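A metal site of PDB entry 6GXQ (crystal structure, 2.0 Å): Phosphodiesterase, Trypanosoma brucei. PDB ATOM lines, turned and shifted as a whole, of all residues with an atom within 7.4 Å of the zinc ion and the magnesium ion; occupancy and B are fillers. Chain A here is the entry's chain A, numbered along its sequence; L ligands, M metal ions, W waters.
Merely in contact with the magnesium ion: His 187 (3.96 Å).
The nearest printed residue that does not touch the magnesium ion is Thr 225 (4.1 Å).
OH of Tyr 110 lies within hydrogen-bond range of ND1 of His 115 (3.5 Å).
ND1 of His 151 lies within hydrogen-bond range of O of Ala 148, at 2.7 Å.
The backbone carbonyl oxygen (O) of Leu 183 sits close to a ring nitrogen (NE2) of His 187, 3.3 Å away.
A ring nitrogen (ND1) of His 187 lies within hydrogen-bond range of the backbone carbonyl oxygen of Leu 153 (2.7 Å).
The zinc ion is bound by NE2 of His 115 (2.1 Å), water W5 (2.1 Å), OD1 of Asp 264 (2.2 Å), OD2 of Asp 152 (2.2 Å), NE2 of His 151 (2.3 Å) and water W1 (2.4 Å).
The zinc ion has six donor atoms within binding distance.
Water W6 bridges the side-chain hydroxyl of Thr 225 (2.6 Å) and the backbone carbonyl oxygen of His 151 (2.6 Å).
Water W2 bridges NE2 of His 187 (2.8 Å) and OE2 of Glu 184 (3.3 Å).
Water W4 bridges OE2 of Glu 184 (2.9 Å) and O of Thr 225 (3.1 Å).
The magnesium ion is bound by OD1 of Asp 152 (2.0 Å), water W3 (2.0 Å), water W2 (2.1 Å), water W6 (2.1 Å), water W5 (2.1 Å) and water W4 (2.1 Å).
The magnesium ion has six donor atoms within binding distance.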
ATOM      1  N   TYR A 110      10.539  36.958  22.947  1.00  0.00           N
ATOM      2  CA  TYR A 110      11.028  35.577  23.152  1.00  0.00           C
ATOM      3  C   TYR A 110      12.539  35.461  22.903  1.00  0.00           C
ATOM      4  O   TYR A 110      13.271  35.069  23.778  1.00  0.00           O
ATOM      5  CB  TYR A 110      10.275  34.587  22.247  1.00  0.00           C
ATOM      6  CG  TYR A 110      10.703  33.164  22.486  1.00  0.00           C
ATOM      7  CD1 TYR A 110      10.246  32.461  23.578  1.00  0.00           C
ATOM      8  CD2 TYR A 110      11.593  32.535  21.636  1.00  0.00           C
ATOM      9  CE1 TYR A 110      10.604  31.139  23.800  1.00  0.00           C
ATOM     10  CE2 TYR A 110      12.011  31.225  21.867  1.00  0.00           C
ATOM     11  CZ  TYR A 110      11.531  30.531  22.976  1.00  0.00           C
ATOM     12  OH  TYR A 110      11.911  29.243  23.210  1.00  0.00           O
ATOM     13  N   HIS A 111      12.992  35.831  21.700  1.00  0.00           N
ATOM     14  CA  HIS A 111      14.387  35.644  21.283  1.00  0.00           C
ATOM     15  C   HIS A 111      15.290  36.724  21.862  1.00  0.00           C
ATOM     16  O   HIS A 111      15.988  37.421  21.119  1.00  0.00           O
ATOM     17  CB  HIS A 111      14.479  35.581  19.765  1.00  0.00           C
ATOM     18  CG  HIS A 111      13.953  34.297  19.214  1.00  0.00           C
ATOM     19  ND1 HIS A 111      12.762  34.209  18.545  1.00  0.00           N
ATOM     20  CD2 HIS A 111      14.426  33.047  19.290  1.00  0.00           C
ATOM     21  CE1 HIS A 111      12.537  32.962  18.203  1.00  0.00           C
ATOM     22  NE2 HIS A 111      13.542  32.245  18.648  1.00  0.00           N
ATOM     23  N   HIS A 115      16.100  33.897  26.812  1.00  0.00           N
ATOM     24  CA  HIS A 115      16.027  32.659  26.045  1.00  0.00           C
ATOM     25  C   HIS A 115      17.387  31.956  26.001  1.00  0.00           C
ATOM     26  O   HIS A 115      17.478  30.743  26.221  1.00  0.00           O
ATOM     27  CB  HIS A 115      15.494  32.919  24.639  1.00  0.00           C
ATOM     28  CG  HIS A 115      15.710  31.793  23.689  1.00  0.00           C
ATOM     29  ND1 HIS A 115      15.088  30.571  23.824  1.00  0.00           N
ATOM     30  CD2 HIS A 115      16.425  31.732  22.556  1.00  0.00           C
ATOM     31  CE1 HIS A 115      15.414  29.805  22.810  1.00  0.00           C
ATOM     32  NE2 HIS A 115      16.230  30.488  22.016  1.00  0.00           N
ATOM     33  N   VAL A 116      18.447  32.706  25.725  1.00  0.00           N
ATOM     34  CA  VAL A 116      19.743  32.045  25.542  1.00  0.00           C
ATOM     35  C   VAL A 116      20.312  31.615  26.898  1.00  0.00           C
ATOM     36  O   VAL A 116      21.000  30.605  26.991  1.00  0.00           O
ATOM     37  CB  VAL A 116      20.712  32.891  24.699  1.00  0.00           C
ATOM     38  CG1 VAL A 116      20.099  33.216  23.350  1.00  0.00           C
ATOM     39  CG2 VAL A 116      21.159  34.164  25.405  1.00  0.00           C
ATOM     40  N   VAL A 119      18.514  28.431  27.552  1.00  0.00           N
ATOM     41  CA  VAL A 119      19.045  27.331  26.739  1.00  0.00           C
ATOM     42  C   VAL A 119      20.353  26.836  27.378  1.00  0.00           C
ATOM     43  O   VAL A 119      20.612  25.649  27.406  1.00  0.00           O
ATOM     44  CB  VAL A 119      19.223  27.755  25.264  1.00  0.00           C
ATOM     45  CG1 VAL A 119      20.041  26.745  24.498  1.00  0.00           C
ATOM     46  CG2 VAL A 119      17.897  27.971  24.558  1.00  0.00           C
ATOM     47  N   ALA A 148      25.393  28.200  23.640  1.00  0.00           N
ATOM     48  CA  ALA A 148      24.026  28.513  24.017  1.00  0.00           C
ATOM     49  C   ALA A 148      23.843  30.033  24.070  1.00  0.00           C
ATOM     50  O   ALA A 148      22.803  30.540  23.675  1.00  0.00           O
ATOM     51  CB  ALA A 148      23.703  27.853  25.327  1.00  0.00           C
ATOM     52  N   HIS A 151      23.820  31.734  20.432  1.00  0.00           N
ATOM     53  CA  HIS A 151      23.157  31.022  19.302  1.00  0.00           C
ATOM     54  C   HIS A 151      22.020  31.806  18.618  1.00  0.00           C
ATOM     55  O   HIS A 151      21.523  31.363  17.566  1.00  0.00           O
ATOM     56  CB  HIS A 151      22.687  29.629  19.720  1.00  0.00           C
ATOM     57  CG  HIS A 151      21.332  29.632  20.329  1.00  0.00           C
ATOM     58  ND1 HIS A 151      21.149  29.875  21.659  1.00  0.00           N
ATOM     59  CD2 HIS A 151      20.116  29.445  19.797  1.00  0.00           C
ATOM     60  CE1 HIS A 151      19.869  29.864  21.930  1.00  0.00           C
ATOM     61  NE2 HIS A 151      19.208  29.604  20.818  1.00  0.00           N
ATOM     62  N   ASP A 152      21.604  32.936  19.225  1.00  0.00           N
ATOM     63  CA  ASP A 152      20.558  33.804  18.693  1.00  0.00           C
ATOM     64  C   ASP A 152      20.953  35.295  18.702  1.00  0.00           C
ATOM     65  O   ASP A 152      20.059  36.148  18.689  1.00  0.00           O
ATOM     66  CB  ASP A 152      19.273  33.630  19.494  1.00  0.00           C
ATOM     67  CG  ASP A 152      18.396  32.495  19.032  1.00  0.00           C
ATOM     68  OD1 ASP A 152      18.476  32.142  17.843  1.00  0.00           O
ATOM     69  OD2 ASP A 152      17.638  31.985  19.878  1.00  0.00           O
ATOM     70  N   LEU A 153      22.254  35.618  18.684  1.00  0.00           N
ATOM     71  CA  LEU A 153      22.726  37.015  18.831  1.00  0.00           C
ATOM     72  C   LEU A 153      22.036  37.900  17.801  1.00  0.00           C
ATOM     73  O   LEU A 153      22.047  37.607  16.611  1.00  0.00           O
ATOM     74  CB  LEU A 153      24.247  37.096  18.626  1.00  0.00           C
ATOM     75  CG  LEU A 153      25.110  36.568  19.769  1.00  0.00           C
ATOM     76  CD1 LEU A 153      26.531  36.322  19.272  1.00  0.00           C
ATOM     77  CD2 LEU A 153      25.111  37.507  20.977  1.00  0.00           C
ATOM     78  N   HIS A 155      18.956  38.631  17.282  1.00  0.00           N
ATOM     79  CA  HIS A 155      17.610  38.275  16.827  1.00  0.00           C
ATOM     80  C   HIS A 155      16.685  39.478  17.000  1.00  0.00           C
ATOM     81  O   HIS A 155      16.709  40.136  18.039  1.00  0.00           O
ATOM     82  CB  HIS A 155      17.062  37.061  17.617  1.00  0.00           C
ATOM     83  CG  HIS A 155      16.075  36.250  16.853  1.00  0.00           C
ATOM     84  ND1 HIS A 155      14.819  36.715  16.552  1.00  0.00           N
ATOM     85  CD2 HIS A 155      16.179  35.014  16.326  1.00  0.00           C
ATOM     86  CE1 HIS A 155      14.187  35.782  15.851  1.00  0.00           C
ATOM     87  NE2 HIS A 155      15.000  34.728  15.706  1.00  0.00           N
ATOM     88  N   LEU A 183      19.253  34.015   9.712  1.00  0.00           N
ATOM     89  CA  LEU A 183      19.576  34.493  11.046  1.00  0.00           C
ATOM     90  C   LEU A 183      20.805  33.750  11.585  1.00  0.00           C
ATOM     91  O   LEU A 183      21.639  34.357  12.285  1.00  0.00           O
ATOM     92  CB  LEU A 183      18.379  34.301  11.971  1.00  0.00           C
ATOM     93  CG  LEU A 183      17.228  35.261  11.759  1.00  0.00           C
ATOM     94  CD1 LEU A 183      15.961  34.748  12.423  1.00  0.00           C
ATOM     95  CD2 LEU A 183      17.580  36.652  12.263  1.00  0.00           C
ATOM     96  N   GLU A 184      20.897  32.449  11.304  1.00  0.00           N
ATOM     97  CA  GLU A 184      21.880  31.584  11.974  1.00  0.00           C
ATOM     98  C   GLU A 184      23.274  32.012  11.511  1.00  0.00           C
ATOM     99  O   GLU A 184      24.209  32.055  12.332  1.00  0.00           O
ATOM    100  CB  GLU A 184      21.639  30.092  11.698  1.00  0.00           C
ATOM    101  CG  GLU A 184      20.358  29.555  12.332  1.00  0.00           C
ATOM    102  CD  GLU A 184      19.035  29.994  11.737  1.00  0.00           C
ATOM    103  OE1 GLU A 184      19.008  30.491  10.563  1.00  0.00           O
ATOM    104  OE2 GLU A 184      18.021  29.851  12.455  1.00  0.00           O
ATOM    105  N   HIS A 187      23.967  35.197  13.451  1.00  0.00           N
ATOM    106  CA  HIS A 187      24.376  34.897  14.822  1.00  0.00           C
ATOM    107  C   HIS A 187      25.863  34.530  14.832  1.00  0.00           C
ATOM    108  O   HIS A 187      26.617  35.017  15.656  1.00  0.00           O
ATOM    109  CB  HIS A 187      23.507  33.794  15.465  1.00  0.00           C
ATOM    110  CG  HIS A 187      22.027  33.979  15.338  1.00  0.00           C
ATOM    111  ND1 HIS A 187      21.409  35.194  15.568  1.00  0.00           N
ATOM    112  CD2 HIS A 187      21.048  33.111  15.026  1.00  0.00           C
ATOM    113  CE1 HIS A 187      20.119  35.061  15.412  1.00  0.00           C
ATOM    114  NE2 HIS A 187      19.868  33.797  15.066  1.00  0.00           N
ATOM    115  N   VAL A 222      25.290  26.285  15.926  1.00  0.00           N
ATOM    116  CA  VAL A 222      24.386  27.404  15.652  1.00  0.00           C
ATOM    117  C   VAL A 222      23.656  27.202  14.311  1.00  0.00           C
ATOM    118  O   VAL A 222      22.462  27.403  14.245  1.00  0.00           O
ATOM    119  CB  VAL A 222      25.111  28.746  15.694  1.00  0.00           C
ATOM    120  CG1 VAL A 222      24.182  29.876  15.276  1.00  0.00           C
ATOM    121  CG2 VAL A 222      25.693  28.995  17.070  1.00  0.00           C
ATOM    122  N   THR A 225      20.574  25.000  14.355  1.00  0.00           N
ATOM    123  CA  THR A 225      19.347  25.493  15.026  1.00  0.00           C
ATOM    124  C   THR A 225      18.290  25.973  14.005  1.00  0.00           C
ATOM    125  O   THR A 225      17.152  26.203  14.377  1.00  0.00           O
ATOM    126  CB  THR A 225      19.631  26.605  16.033  1.00  0.00           C
ATOM    127  OG1 THR A 225      20.241  27.747  15.424  1.00  0.00           O
ATOM    128  CG2 THR A 225      20.509  26.140  17.167  1.00  0.00           C
ATOM    129  N   ASP A 226      18.639  26.113  12.722  1.00  0.00           N
ATOM    130  CA  ASP A 226      17.659  26.422  11.679  1.00  0.00           C
ATOM    131  C   ASP A 226      16.677  25.261  11.576  1.00  0.00           C
ATOM    132  O   ASP A 226      17.014  24.158  11.119  1.00  0.00           O
ATOM    133  CB  ASP A 226      18.330  26.709  10.332  1.00  0.00           C
ATOM    134  CG  ASP A 226      17.358  26.989   9.179  1.00  0.00           C
ATOM    135  OD1 ASP A 226      16.150  26.825   9.380  1.00  0.00           O
ATOM    136  OD2 ASP A 226      17.835  27.349   8.089  1.00  0.00           O
ATOM    137  N   MET A 227      15.432  25.506  11.977  1.00  0.00           N
ATOM    138  CA  MET A 227      14.408  24.467  12.035  1.00  0.00           C
ATOM    139  C   MET A 227      14.071  23.925  10.633  1.00  0.00           C
ATOM    140  O   MET A 227      13.452  22.878  10.545  1.00  0.00           O
ATOM    141  CB  MET A 227      13.117  24.965  12.705  1.00  0.00           C
ATOM    142  CG  MET A 227      13.215  25.051  14.211  1.00  0.00           C
ATOM    143  SD  MET A 227      13.730  23.468  14.982  1.00  0.00           S
ATOM    144  CE  MET A 227      12.228  22.507  14.769  1.00  0.00           C
ATOM    145  N   LEU A 260      22.167  21.272  21.369  1.00  0.00           N
ATOM    146  CA  LEU A 260      21.757  22.710  21.210  1.00  0.00           C
ATOM    147  C   LEU A 260      20.327  22.777  20.684  1.00  0.00           C
ATOM    148  O   LEU A 260      19.518  23.519  21.191  1.00  0.00           O
ATOM    149  CB  LEU A 260      22.695  23.476  20.273  1.00  0.00           C
ATOM    150  CG  LEU A 260      22.354  24.964  20.093  1.00  0.00           C
ATOM    151  CD1 LEU A 260      22.284  25.710  21.417  1.00  0.00           C
ATOM    152  CD2 LEU A 260      23.337  25.641  19.181  1.00  0.00           C
ATOM    153  N   GLY A 263      17.957  21.942  23.498  1.00  0.00           N
ATOM    154  CA  GLY A 263      17.804  23.062  24.396  1.00  0.00           C
ATOM    155  C   GLY A 263      16.927  24.151  23.793  1.00  0.00           C
ATOM    156  O   GLY A 263      16.118  24.779  24.460  1.00  0.00           O
ATOM    157  N   ASP A 264      17.069  24.326  22.482  1.00  0.00           N
ATOM    158  CA  ASP A 264      16.358  25.334  21.753  1.00  0.00           C
ATOM    159  C   ASP A 264      14.838  25.054  21.715  1.00  0.00           C
ATOM    160  O   ASP A 264      14.047  25.986  21.636  1.00  0.00           O
ATOM    161  CB  ASP A 264      16.887  25.457  20.334  1.00  0.00           C
ATOM    162  CG  ASP A 264      16.763  26.864  19.773  1.00  0.00           C
ATOM    163  OD1 ASP A 264      16.671  27.794  20.577  1.00  0.00           O
ATOM    164  OD2 ASP A 264      16.809  27.014  18.540  1.00  0.00           O
ATOM    165  N   ILE A 265      14.425  23.784  21.753  1.00  0.00           N
ATOM    166  CA  ILE A 265      12.985  23.443  21.780  1.00  0.00           C
ATOM    167  C   ILE A 265      12.591  22.778  23.107  1.00  0.00           C
ATOM    168  O   ILE A 265      11.688  21.941  23.135  1.00  0.00           O
ATOM    169  CB  ILE A 265      12.611  22.579  20.557  1.00  0.00           C
ATOM    170  CG1 ILE A 265      13.373  21.254  20.516  1.00  0.00           C
ATOM    171  CG2 ILE A 265      12.798  23.358  19.277  1.00  0.00           C
ATOM    172  CD1 ILE A 265      12.787  20.298  19.530  1.00  0.00           C
HETATM  173  C1  LIG L   1       7.117  27.323  23.462  1.00  0.00           C
HETATM  174  C2  LIG L   1       2.877  25.132  16.495  1.00  0.00           C
HETATM  175  C3  LIG L   1       2.452  23.900  16.019  1.00  0.00           C
HETATM  176  C4  LIG L   1       5.023  24.723  15.472  1.00  0.00           C
HETATM  177  C5  LIG L   1       4.173  25.546  16.210  1.00  0.00           C
HETATM  178  C6  LIG L   1       2.921  26.979  19.295  1.00  0.00           C
HETATM  179  C7  LIG L   1       1.936  26.022  17.281  1.00  0.00           C
HETATM  180  C8  LIG L   1       3.309  23.089  15.284  1.00  0.00           C
HETATM  181  C9  LIG L   1       4.594  23.505  15.013  1.00  0.00           C
HETATM  182  C10 LIG L   1       9.847  27.381  17.514  1.00  0.00           C
HETATM  183  C11 LIG L   1       9.276  26.326  14.159  1.00  0.00           C
HETATM  184  C12 LIG L   1       7.540  26.941  21.118  1.00  0.00           C
HETATM  185  C13 LIG L   1       9.023  24.892  14.600  1.00  0.00           C
HETATM  186  C14 LIG L   1       8.025  27.034  13.662  1.00  0.00           C
HETATM  187  C15 LIG L   1      11.050  27.829  15.056  1.00  0.00           C
HETATM  188  C16 LIG L   1      11.573  28.636  16.217  1.00  0.00           C
HETATM  189  C17 LIG L   1      13.039  29.073  16.063  1.00  0.00           C
HETATM  190  C18 LIG L   1      13.990  27.973  16.372  1.00  0.00           C
HETATM  191  C19 LIG L   1      13.664  26.895  17.061  1.00  0.00           C
HETATM  192  C20 LIG L   1      12.298  26.630  17.608  1.00  0.00           C
HETATM  193  C21 LIG L   1      11.322  27.826  17.503  1.00  0.00           C
HETATM  194  C22 LIG L   1       8.935  27.032  21.202  1.00  0.00           C
HETATM  195  C23 LIG L   1       9.700  27.170  20.055  1.00  0.00           C
HETATM  196  C24 LIG L   1       9.103  27.246  18.800  1.00  0.00           C
HETATM  197  C25 LIG L   1       7.707  27.158  18.706  1.00  0.00           C
HETATM  198  C26 LIG L   1       6.927  26.998  19.846  1.00  0.00           C
HETATM  199  C27 LIG L   1       5.503  26.938  19.723  1.00  0.00           C
HETATM  200  C28 LIG L   1       4.321  26.979  19.569  1.00  0.00           C
HETATM  201  N1  LIG L   1       2.622  27.100  17.991  1.00  0.00           N
HETATM  202  N2  LIG L   1       9.185  27.128  16.437  1.00  0.00           N
HETATM  203  N3  LIG L   1       9.874  27.122  15.264  1.00  0.00           N
HETATM  204  O1  LIG L   1       6.702  26.803  22.196  1.00  0.00           O
HETATM  205  O2  LIG L   1       2.106  26.908  20.203  1.00  0.00           O
HETATM  206  O3  LIG L   1      11.629  27.772  13.983  1.00  0.00           O
HETATM  207 ZN    ZN M   1      17.069  29.879  20.173  1.00  0.00          ZN
HETATM  208 MG    MG M   2      17.731  30.809  16.540  1.00  0.00          MG
HETATM  209  O   HOH W   1      14.929  29.960  19.170  1.00  0.00           O
HETATM  210  O   HOH W   2      17.664  32.061  14.914  1.00  0.00           O
HETATM  211  O   HOH W   3      15.754  31.190  16.742  1.00  0.00           O
HETATM  212  O   HOH W   4      17.473  29.170  15.211  1.00  0.00           O
HETATM  213  O   HOH W   5      17.342  29.480  18.089  1.00  0.00           O
HETATM  214  O   HOH W   6      19.645  30.158  16.172  1.00  0.00           O
